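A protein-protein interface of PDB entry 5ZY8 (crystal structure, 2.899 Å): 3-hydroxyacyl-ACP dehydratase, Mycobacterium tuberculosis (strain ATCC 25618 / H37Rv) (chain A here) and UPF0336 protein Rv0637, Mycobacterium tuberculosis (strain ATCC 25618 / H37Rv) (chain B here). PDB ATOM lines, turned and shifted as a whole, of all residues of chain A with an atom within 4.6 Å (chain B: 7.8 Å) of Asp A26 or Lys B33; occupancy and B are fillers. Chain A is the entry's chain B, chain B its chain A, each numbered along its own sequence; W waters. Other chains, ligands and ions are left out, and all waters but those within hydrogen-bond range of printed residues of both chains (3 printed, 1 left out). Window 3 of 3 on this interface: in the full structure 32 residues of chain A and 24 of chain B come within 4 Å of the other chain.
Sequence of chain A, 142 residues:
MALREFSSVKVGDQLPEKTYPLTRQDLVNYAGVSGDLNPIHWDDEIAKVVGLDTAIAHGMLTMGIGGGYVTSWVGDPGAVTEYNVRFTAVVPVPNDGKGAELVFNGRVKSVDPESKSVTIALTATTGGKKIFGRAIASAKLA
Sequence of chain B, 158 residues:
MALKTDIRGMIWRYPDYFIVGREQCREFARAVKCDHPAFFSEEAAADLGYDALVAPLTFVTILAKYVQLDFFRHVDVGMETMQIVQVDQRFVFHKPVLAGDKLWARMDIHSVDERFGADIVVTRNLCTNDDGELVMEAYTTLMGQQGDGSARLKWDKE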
ATOM      1  N   TYR A  20     -16.164 -12.348 -11.102  1.00  0.00           N
ATOM      2  CA  TYR A  20     -17.366 -12.472 -11.899  1.00  0.00           C
ATOM      3  C   TYR A  20     -17.418 -11.326 -12.893  1.00  0.00           C
ATOM      4  O   TYR A  20     -17.276 -10.162 -12.488  1.00  0.00           O
ATOM      5  CB  TYR A  20     -18.634 -12.411 -11.008  1.00  0.00           C
ATOM      6  CG  TYR A  20     -18.799 -13.519 -10.007  1.00  0.00           C
ATOM      7  CD1 TYR A  20     -18.112 -13.485  -8.803  1.00  0.00           C
ATOM      8  CD2 TYR A  20     -19.677 -14.577 -10.230  1.00  0.00           C
ATOM      9  CE1 TYR A  20     -18.249 -14.497  -7.864  1.00  0.00           C
ATOM     10  CE2 TYR A  20     -19.835 -15.594  -9.278  1.00  0.00           C
ATOM     11  CZ  TYR A  20     -19.110 -15.540  -8.103  1.00  0.00           C
ATOM     12  OH  TYR A  20     -19.242 -16.504  -7.140  1.00  0.00           O
ATOM     13  N   PRO A  21     -17.669 -11.587 -14.169  1.00  0.00           N
ATOM     14  CA  PRO A  21     -17.877 -10.483 -15.099  1.00  0.00           C
ATOM     15  C   PRO A  21     -19.290  -9.961 -14.888  1.00  0.00           C
ATOM     16  O   PRO A  21     -20.228 -10.708 -14.580  1.00  0.00           O
ATOM     17  CB  PRO A  21     -17.666 -11.124 -16.479  1.00  0.00           C
ATOM     18  CG  PRO A  21     -18.076 -12.516 -16.292  1.00  0.00           C
ATOM     19  CD  PRO A  21     -17.828 -12.893 -14.835  1.00  0.00           C
ATOM     20  N   LEU A  22     -19.459  -8.672 -15.158  1.00  0.00           N
ATOM     21  CA  LEU A  22     -20.778  -8.039 -15.095  1.00  0.00           C
ATOM     22  C   LEU A  22     -20.949  -7.122 -16.290  1.00  0.00           C
ATOM     23  O   LEU A  22     -20.137  -6.219 -16.489  1.00  0.00           O
ATOM     24  CB  LEU A  22     -20.933  -7.294 -13.744  1.00  0.00           C
ATOM     25  CG  LEU A  22     -21.889  -7.825 -12.673  1.00  0.00           C
ATOM     26  CD1 LEU A  22     -22.138  -6.830 -11.580  1.00  0.00           C
ATOM     27  CD2 LEU A  22     -23.128  -8.091 -13.423  1.00  0.00           C
ATOM     28  N   THR A  23     -22.009  -7.340 -17.064  1.00  0.00           N
ATOM     29  CA  THR A  23     -22.233  -6.559 -18.272  1.00  0.00           C
ATOM     30  C   THR A  23     -23.546  -5.792 -18.162  1.00  0.00           C
ATOM     31  O   THR A  23     -24.352  -6.020 -17.259  1.00  0.00           O
ATOM     32  CB  THR A  23     -22.306  -7.438 -19.528  1.00  0.00           C
ATOM     33  OG1 THR A  23     -23.449  -8.304 -19.440  1.00  0.00           O
ATOM     34  CG2 THR A  23     -21.058  -8.310 -19.647  1.00  0.00           C
ATOM     35  N   ARG A  24     -23.753  -4.870 -19.111  1.00  0.00           N
ATOM     36  CA  ARG A  24     -24.977  -4.085 -19.109  1.00  0.00           C
ATOM     37  C   ARG A  24     -26.187  -4.988 -19.273  1.00  0.00           C
ATOM     38  O   ARG A  24     -27.223  -4.781 -18.629  1.00  0.00           O
ATOM     39  CB  ARG A  24     -24.917  -3.031 -20.214  1.00  0.00           C
ATOM     40  CG  ARG A  24     -26.106  -2.093 -20.210  1.00  0.00           C
ATOM     41  CD  ARG A  24     -26.166  -1.309 -18.910  1.00  0.00           C
ATOM     42  NE  ARG A  24     -24.985  -0.472 -18.756  1.00  0.00           N
ATOM     43  CZ  ARG A  24     -24.896   0.773 -19.215  1.00  0.00           C
ATOM     44  NH1 ARG A  24     -25.889   1.291 -19.922  1.00  0.00           N
ATOM     45  NH2 ARG A  24     -23.783   1.466 -19.033  1.00  0.00           N
ATOM     46  N   GLN A  25     -26.050  -6.024 -20.108  1.00  0.00           N
ATOM     47  CA  GLN A  25     -27.124  -6.990 -20.294  1.00  0.00           C
ATOM     48  C   GLN A  25     -27.526  -7.631 -18.972  1.00  0.00           C
ATOM     49  O   GLN A  25     -28.708  -7.916 -18.733  1.00  0.00           O
ATOM     50  CB  GLN A  25     -26.655  -8.059 -21.271  1.00  0.00           C
ATOM     51  CG  GLN A  25     -27.658  -9.100 -21.593  1.00  0.00           C
ATOM     52  CD  GLN A  25     -27.223  -9.910 -22.770  1.00  0.00           C
ATOM     53  OE1 GLN A  25     -27.358  -9.484 -23.921  1.00  0.00           O
ATOM     54  NE2 GLN A  25     -26.649 -11.074 -22.496  1.00  0.00           N
ATOM     55  N   ASP A  26     -26.550  -7.876 -18.102  1.00  0.00           N
ATOM     56  CA  ASP A  26     -26.862  -8.437 -16.798  1.00  0.00           C
ATOM     57  C   ASP A  26     -27.708  -7.475 -15.966  1.00  0.00           C
ATOM     58  O   ASP A  26     -28.636  -7.900 -15.268  1.00  0.00           O
ATOM     59  CB  ASP A  26     -25.575  -8.787 -16.055  1.00  0.00           C
ATOM     60  CG  ASP A  26     -24.758  -9.834 -16.773  1.00  0.00           C
ATOM     61  OD1 ASP A  26     -25.351 -10.766 -17.347  1.00  0.00           O
ATOM     62  OD2 ASP A  26     -23.512  -9.757 -16.709  1.00  0.00           O
ATOM     63  N   LEU A  27     -27.412  -6.177 -16.035  1.00  0.00           N
ATOM     64  CA  LEU A  27     -28.174  -5.209 -15.255  1.00  0.00           C
ATOM     65  C   LEU A  27     -29.617  -5.106 -15.745  1.00  0.00           C
ATOM     66  O   LEU A  27     -30.557  -5.100 -14.933  1.00  0.00           O
ATOM     67  CB  LEU A  27     -27.471  -3.848 -15.316  1.00  0.00           C
ATOM     68  CG  LEU A  27     -26.370  -3.552 -14.293  1.00  0.00           C
ATOM     69  CD1 LEU A  27     -25.322  -4.660 -14.255  1.00  0.00           C
ATOM     70  CD2 LEU A  27     -25.729  -2.219 -14.598  1.00  0.00           C
ATOM     71  N   VAL A  28     -29.820  -5.048 -17.066  1.00  0.00           N
ATOM     72  CA  VAL A  28     -31.182  -4.979 -17.599  1.00  0.00           C
ATOM     73  C   VAL A  28     -31.930  -6.251 -17.219  1.00  0.00           C
ATOM     74  O   VAL A  28     -33.131  -6.215 -16.913  1.00  0.00           O
ATOM     75  CB  VAL A  28     -31.203  -4.670 -19.106  1.00  0.00           C
ATOM     76  CG1 VAL A  28     -30.270  -5.544 -19.861  1.00  0.00           C
ATOM     77  CG2 VAL A  28     -32.601  -4.782 -19.677  1.00  0.00           C
ATOM     78  N   ASN A  29     -31.260  -7.404 -17.317  1.00  0.00           N
ATOM     79  CA  ASN A  29     -31.895  -8.645 -16.885  1.00  0.00           C
ATOM     80  C   ASN A  29     -32.297  -8.560 -15.414  1.00  0.00           C
ATOM     81  O   ASN A  29     -33.445  -8.858 -15.058  1.00  0.00           O
ATOM     82  CB  ASN A  29     -30.938  -9.806 -17.099  1.00  0.00           C
ATOM     83  CG  ASN A  29     -31.543 -11.140 -16.721  1.00  0.00           C
ATOM     84  OD1 ASN A  29     -32.607 -11.525 -17.224  1.00  0.00           O
ATOM     85  ND2 ASN A  29     -30.882 -11.849 -15.812  1.00  0.00           N
ATOM     86  N   TYR A  30     -31.379  -8.114 -14.543  1.00  0.00           N
ATOM     87  CA  TYR A  30     -31.686  -8.088 -13.109  1.00  0.00           C
ATOM     88  C   TYR A  30     -32.830  -7.134 -12.801  1.00  0.00           C
ATOM     89  O   TYR A  30     -33.640  -7.397 -11.906  1.00  0.00           O
ATOM     90  CB  TYR A  30     -30.467  -7.740 -12.247  1.00  0.00           C
ATOM     91  CG  TYR A  30     -30.768  -7.894 -10.760  1.00  0.00           C
ATOM     92  CD1 TYR A  30     -30.761  -9.134 -10.119  1.00  0.00           C
ATOM     93  CD2 TYR A  30     -31.113  -6.774 -10.010  1.00  0.00           C
ATOM     94  CE1 TYR A  30     -31.049  -9.239  -8.748  1.00  0.00           C
ATOM     95  CE2 TYR A  30     -31.416  -6.871  -8.674  1.00  0.00           C
ATOM     96  CZ  TYR A  30     -31.379  -8.099  -8.041  1.00  0.00           C
ATOM     97  OH  TYR A  30     -31.703  -8.148  -6.706  1.00  0.00           O
ATOM     98  N   ILE A  65     -24.783 -11.902  -5.981  1.00  0.00           N
ATOM     99  CA  ILE A  65     -23.586 -12.609  -6.417  1.00  0.00           C
ATOM    100  C   ILE A  65     -22.821 -13.127  -5.206  1.00  0.00           C
ATOM    101  O   ILE A  65     -22.345 -14.268  -5.194  1.00  0.00           O
ATOM    102  CB  ILE A  65     -22.715 -11.704  -7.296  1.00  0.00           C
ATOM    103  CG1 ILE A  65     -23.461 -11.371  -8.584  1.00  0.00           C
ATOM    104  CG2 ILE A  65     -21.415 -12.396  -7.620  1.00  0.00           C
ATOM    105  CD1 ILE A  65     -22.771 -10.324  -9.431  1.00  0.00           C
ATOM    106  N   GLU B  27     -34.584 -18.461 -12.426  1.00  0.00           N
ATOM    107  CA  GLU B  27     -34.166 -17.321 -13.234  1.00  0.00           C
ATOM    108  C   GLU B  27     -33.414 -16.301 -12.387  1.00  0.00           C
ATOM    109  O   GLU B  27     -32.367 -15.789 -12.801  1.00  0.00           O
ATOM    110  CB  GLU B  27     -35.384 -16.687 -13.905  1.00  0.00           C
ATOM    111  CG  GLU B  27     -35.963 -17.455 -15.110  1.00  0.00           C
ATOM    112  CD  GLU B  27     -34.981 -17.629 -16.259  1.00  0.00           C
ATOM    113  OE1 GLU B  27     -34.070 -16.783 -16.396  1.00  0.00           O
ATOM    114  OE2 GLU B  27     -35.130 -18.595 -17.046  1.00  0.00           O
ATOM    115  N   PHE B  28     -33.915 -16.031 -11.176  1.00  0.00           N
ATOM    116  CA  PHE B  28     -33.213 -15.166 -10.229  1.00  0.00           C
ATOM    117  C   PHE B  28     -31.816 -15.697  -9.925  1.00  0.00           C
ATOM    118  O   PHE B  28     -30.834 -14.946  -9.939  1.00  0.00           O
ATOM    119  CB  PHE B  28     -34.042 -15.051  -8.946  1.00  0.00           C
ATOM    120  CG  PHE B  28     -33.605 -13.955  -8.020  1.00  0.00           C
ATOM    121  CD1 PHE B  28     -32.546 -14.155  -7.132  1.00  0.00           C
ATOM    122  CD2 PHE B  28     -34.252 -12.729  -8.013  1.00  0.00           C
ATOM    123  CE1 PHE B  28     -32.138 -13.157  -6.259  1.00  0.00           C
ATOM    124  CE2 PHE B  28     -33.841 -11.722  -7.135  1.00  0.00           C
ATOM    125  CZ  PHE B  28     -32.783 -11.942  -6.258  1.00  0.00           C
ATOM    126  N   ALA B  29     -31.709 -16.997  -9.647  1.00  0.00           N
ATOM    127  CA  ALA B  29     -30.409 -17.589  -9.355  1.00  0.00           C
ATOM    128  C   ALA B  29     -29.429 -17.327 -10.488  1.00  0.00           C
ATOM    129  O   ALA B  29     -28.274 -16.944 -10.258  1.00  0.00           O
ATOM    130  CB  ALA B  29     -30.562 -19.087  -9.104  1.00  0.00           C
ATOM    131  N   ARG B  30     -29.865 -17.565 -11.726  1.00  0.00           N
ATOM    132  CA  ARG B  30     -28.998 -17.332 -12.874  1.00  0.00           C
ATOM    133  C   ARG B  30     -28.696 -15.848 -13.054  1.00  0.00           C
ATOM    134  O   ARG B  30     -27.626 -15.487 -13.566  1.00  0.00           O
ATOM    135  CB  ARG B  30     -29.637 -17.917 -14.133  1.00  0.00           C
ATOM    136  CG  ARG B  30     -28.689 -18.757 -14.940  1.00  0.00           C
ATOM    137  CD  ARG B  30     -29.405 -19.437 -16.080  1.00  0.00           C
ATOM    138  NE  ARG B  30     -30.466 -20.336 -15.620  1.00  0.00           N
ATOM    139  CZ  ARG B  30     -31.760 -20.165 -15.891  1.00  0.00           C
ATOM    140  NH1 ARG B  30     -32.155 -19.127 -16.629  1.00  0.00           N
ATOM    141  NH2 ARG B  30     -32.656 -21.035 -15.433  1.00  0.00           N
ATOM    142  N   ALA B  31     -29.623 -14.979 -12.635  1.00  0.00           N
ATOM    143  CA  ALA B  31     -29.408 -13.549 -12.778  1.00  0.00           C
ATOM    144  C   ALA B  31     -28.313 -13.056 -11.848  1.00  0.00           C
ATOM    145  O   ALA B  31     -27.617 -12.093 -12.178  1.00  0.00           O
ATOM    146  CB  ALA B  31     -30.704 -12.792 -12.514  1.00  0.00           C
ATOM    147  N   VAL B  32     -28.115 -13.706 -10.707  1.00  0.00           N
ATOM    148  CA  VAL B  32     -27.056 -13.314  -9.787  1.00  0.00           C
ATOM    149  C   VAL B  32     -25.926 -14.343  -9.788  1.00  0.00           C
ATOM    150  O   VAL B  32     -25.172 -14.442  -8.822  1.00  0.00           O
ATOM    151  CB  VAL B  32     -27.603 -13.065  -8.372  1.00  0.00           C
ATOM    152  CG1 VAL B  32     -28.744 -12.075  -8.429  1.00  0.00           C
ATOM    153  CG2 VAL B  32     -28.013 -14.379  -7.680  1.00  0.00           C
ATOM    154  N   LYS B  33     -25.829 -15.129 -10.866  1.00  0.00           N
ATOM    155  CA  LYS B  33     -24.650 -15.928 -11.200  1.00  0.00           C
ATOM    156  C   LYS B  33     -24.386 -17.065 -10.207  1.00  0.00           C
ATOM    157  O   LYS B  33     -23.255 -17.546 -10.092  1.00  0.00           O
ATOM    158  CB  LYS B  33     -23.413 -15.038 -11.349  1.00  0.00           C
ATOM    159  CG  LYS B  33     -23.689 -13.790 -12.176  1.00  0.00           C
ATOM    160  CD  LYS B  33     -22.542 -13.418 -13.099  1.00  0.00           C
ATOM    161  CE  LYS B  33     -23.023 -12.456 -14.181  1.00  0.00           C
ATOM    162  NZ  LYS B  33     -24.101 -13.066 -15.024  1.00  0.00           N
ATOM    163  N   CYS B  34     -25.417 -17.566  -9.532  1.00  0.00           N
ATOM    164  CA  CYS B  34     -25.254 -18.803  -8.777  1.00  0.00           C
ATOM    165  C   CYS B  34     -24.942 -19.966  -9.710  1.00  0.00           C
ATOM    166  O   CYS B  34     -25.374 -19.995 -10.867  1.00  0.00           O
ATOM    167  CB  CYS B  34     -26.519 -19.133  -7.987  1.00  0.00           C
ATOM    168  SG  CYS B  34     -27.037 -17.894  -6.821  1.00  0.00           S
ATOM    169  N   ASP B  35     -24.133 -20.913  -9.220  1.00  0.00           N
ATOM    170  CA  ASP B  35     -23.922 -22.150  -9.962  1.00  0.00           C
ATOM    171  C   ASP B  35     -24.083 -23.426  -9.137  1.00  0.00           C
ATOM    172  O   ASP B  35     -23.830 -24.513  -9.669  1.00  0.00           O
ATOM    173  CB  ASP B  35     -22.540 -22.177 -10.632  1.00  0.00           C
ATOM    174  CG  ASP B  35     -21.469 -21.614  -9.764  1.00  0.00           C
ATOM    175  OD1 ASP B  35     -21.448 -21.967  -8.559  1.00  0.00           O
ATOM    176  OD2 ASP B  35     -20.643 -20.840 -10.301  1.00  0.00           O
ATOM    177  N   HIS B  36     -24.485 -23.340  -7.876  1.00  0.00           N
ATOM    178  CA  HIS B  36     -24.713 -24.556  -7.101  1.00  0.00           C
ATOM    179  C   HIS B  36     -25.954 -25.259  -7.639  1.00  0.00           C
ATOM    180  O   HIS B  36     -27.011 -24.627  -7.766  1.00  0.00           O
ATOM    181  CB  HIS B  36     -24.891 -24.238  -5.622  1.00  0.00           C
ATOM    182  CG  HIS B  36     -24.735 -25.428  -4.728  1.00  0.00           C
ATOM    183  ND1 HIS B  36     -25.595 -26.502  -4.766  1.00  0.00           N
ATOM    184  CD2 HIS B  36     -23.844 -25.695  -3.744  1.00  0.00           C
ATOM    185  CE1 HIS B  36     -25.227 -27.386  -3.858  1.00  0.00           C
ATOM    186  NE2 HIS B  36     -24.168 -26.922  -3.222  1.00  0.00           N
ATOM    187  N   PHE B  39     -29.697 -24.856  -6.437  1.00  0.00           N
ATOM    188  CA  PHE B  39     -30.533 -23.744  -6.884  1.00  0.00           C
ATOM    189  C   PHE B  39     -31.397 -24.110  -8.082  1.00  0.00           C
ATOM    190  O   PHE B  39     -32.420 -23.452  -8.313  1.00  0.00           O
ATOM    191  CB  PHE B  39     -29.668 -22.544  -7.260  1.00  0.00           C
ATOM    192  CG  PHE B  39     -29.004 -21.885  -6.086  1.00  0.00           C
ATOM    193  CD1 PHE B  39     -29.762 -21.392  -5.028  1.00  0.00           C
ATOM    194  CD2 PHE B  39     -27.612 -21.799  -6.012  1.00  0.00           C
ATOM    195  CE1 PHE B  39     -29.143 -20.802  -3.941  1.00  0.00           C
ATOM    196  CE2 PHE B  39     -27.002 -21.218  -4.929  1.00  0.00           C
ATOM    197  CZ  PHE B  39     -27.762 -20.722  -3.894  1.00  0.00           C
ATOM    198  N   PHE B  40     -31.012 -25.140  -8.845  1.00  0.00           N
ATOM    199  CA  PHE B  40     -31.631 -25.422 -10.134  1.00  0.00           C
ATOM    200  C   PHE B  40     -32.248 -26.808 -10.246  1.00  0.00           C
ATOM    201  O   PHE B  40     -33.191 -26.981 -11.022  1.00  0.00           O
ATOM    202  CB  PHE B  40     -30.602 -25.267 -11.269  1.00  0.00           C
ATOM    203  CG  PHE B  40     -29.913 -23.953 -11.285  1.00  0.00           C
ATOM    204  CD1 PHE B  40     -30.468 -22.876 -11.962  1.00  0.00           C
ATOM    205  CD2 PHE B  40     -28.712 -23.773 -10.619  1.00  0.00           C
ATOM    206  CE1 PHE B  40     -29.834 -21.636 -11.978  1.00  0.00           C
ATOM    207  CE2 PHE B  40     -28.073 -22.543 -10.625  1.00  0.00           C
ATOM    208  CZ  PHE B  40     -28.639 -21.469 -11.309  1.00  0.00           C
HETATM  209  O   HOH W   1     -28.600 -10.438 -14.373  1.00  0.00           O
HETATM  210  O   HOH W   2     -21.590 -18.270  -7.815  1.00  0.00           O
HETATM  211  O   HOH W   3     -31.873 -14.686 -15.575  1.00  0.00           O
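OD1 of Asp A26 is in salt-bridge range of NZ of Lys B33, at 3.5 Å.
The side-chain carboxylate (OD2) of Asp A26 sits at hydrogen-bond distance from the backbone NH (N) of Thr A23.
Among the printed residues, merely in contact across the chains: Tyr A20 with Lys B33, Pro A21 with Lys B33, Asn A29 with Ala B31, Tyr A30 with Phe B28, Tyr A30 with Val B32 and Ile A65 with Val B32.
Of the printed residues of chain B, Tyr A20 touches Lys B33 (3.9 Å).
Of chain B, only Lys B33 comes within 4 Å of Asp A26.
Of the printed residues of chain B, Tyr A30 touches Phe B28 (3.97 Å) and Val B32 (3.7 Å).
Lys B33 touches just these residues of chain A: Tyr A20, Pro A21 and Asp A26.
Cys B34 touches none of the printed residues of chain A.
Hydrophobic or aromatic side chains of chain B within 4 Å of the printed part of chain A: Phe B28, Ala B31 and Val B32.
Printed residues of chain A that touch a printed residue of chain B: Tyr A20, Pro A21, Asp A26, Asn A29, Tyr A30 and Ile A65.
Water W1 lies within hydrogen-bond range of O of Asp A26 (2.7 Å), O of Ala B31 (2.9 Å) and ND2 of Asn A29 (3.0 Å).
Water W2 bridges O of Lys B33 (2.9 Å) and OH of Tyr A20 (3.0 Å).
Water W3 bridges the side-chain amide nitrogen of Asn A29 (3.0 Å) and the backbone carbonyl oxygen of Glu B27 (3.0 Å).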
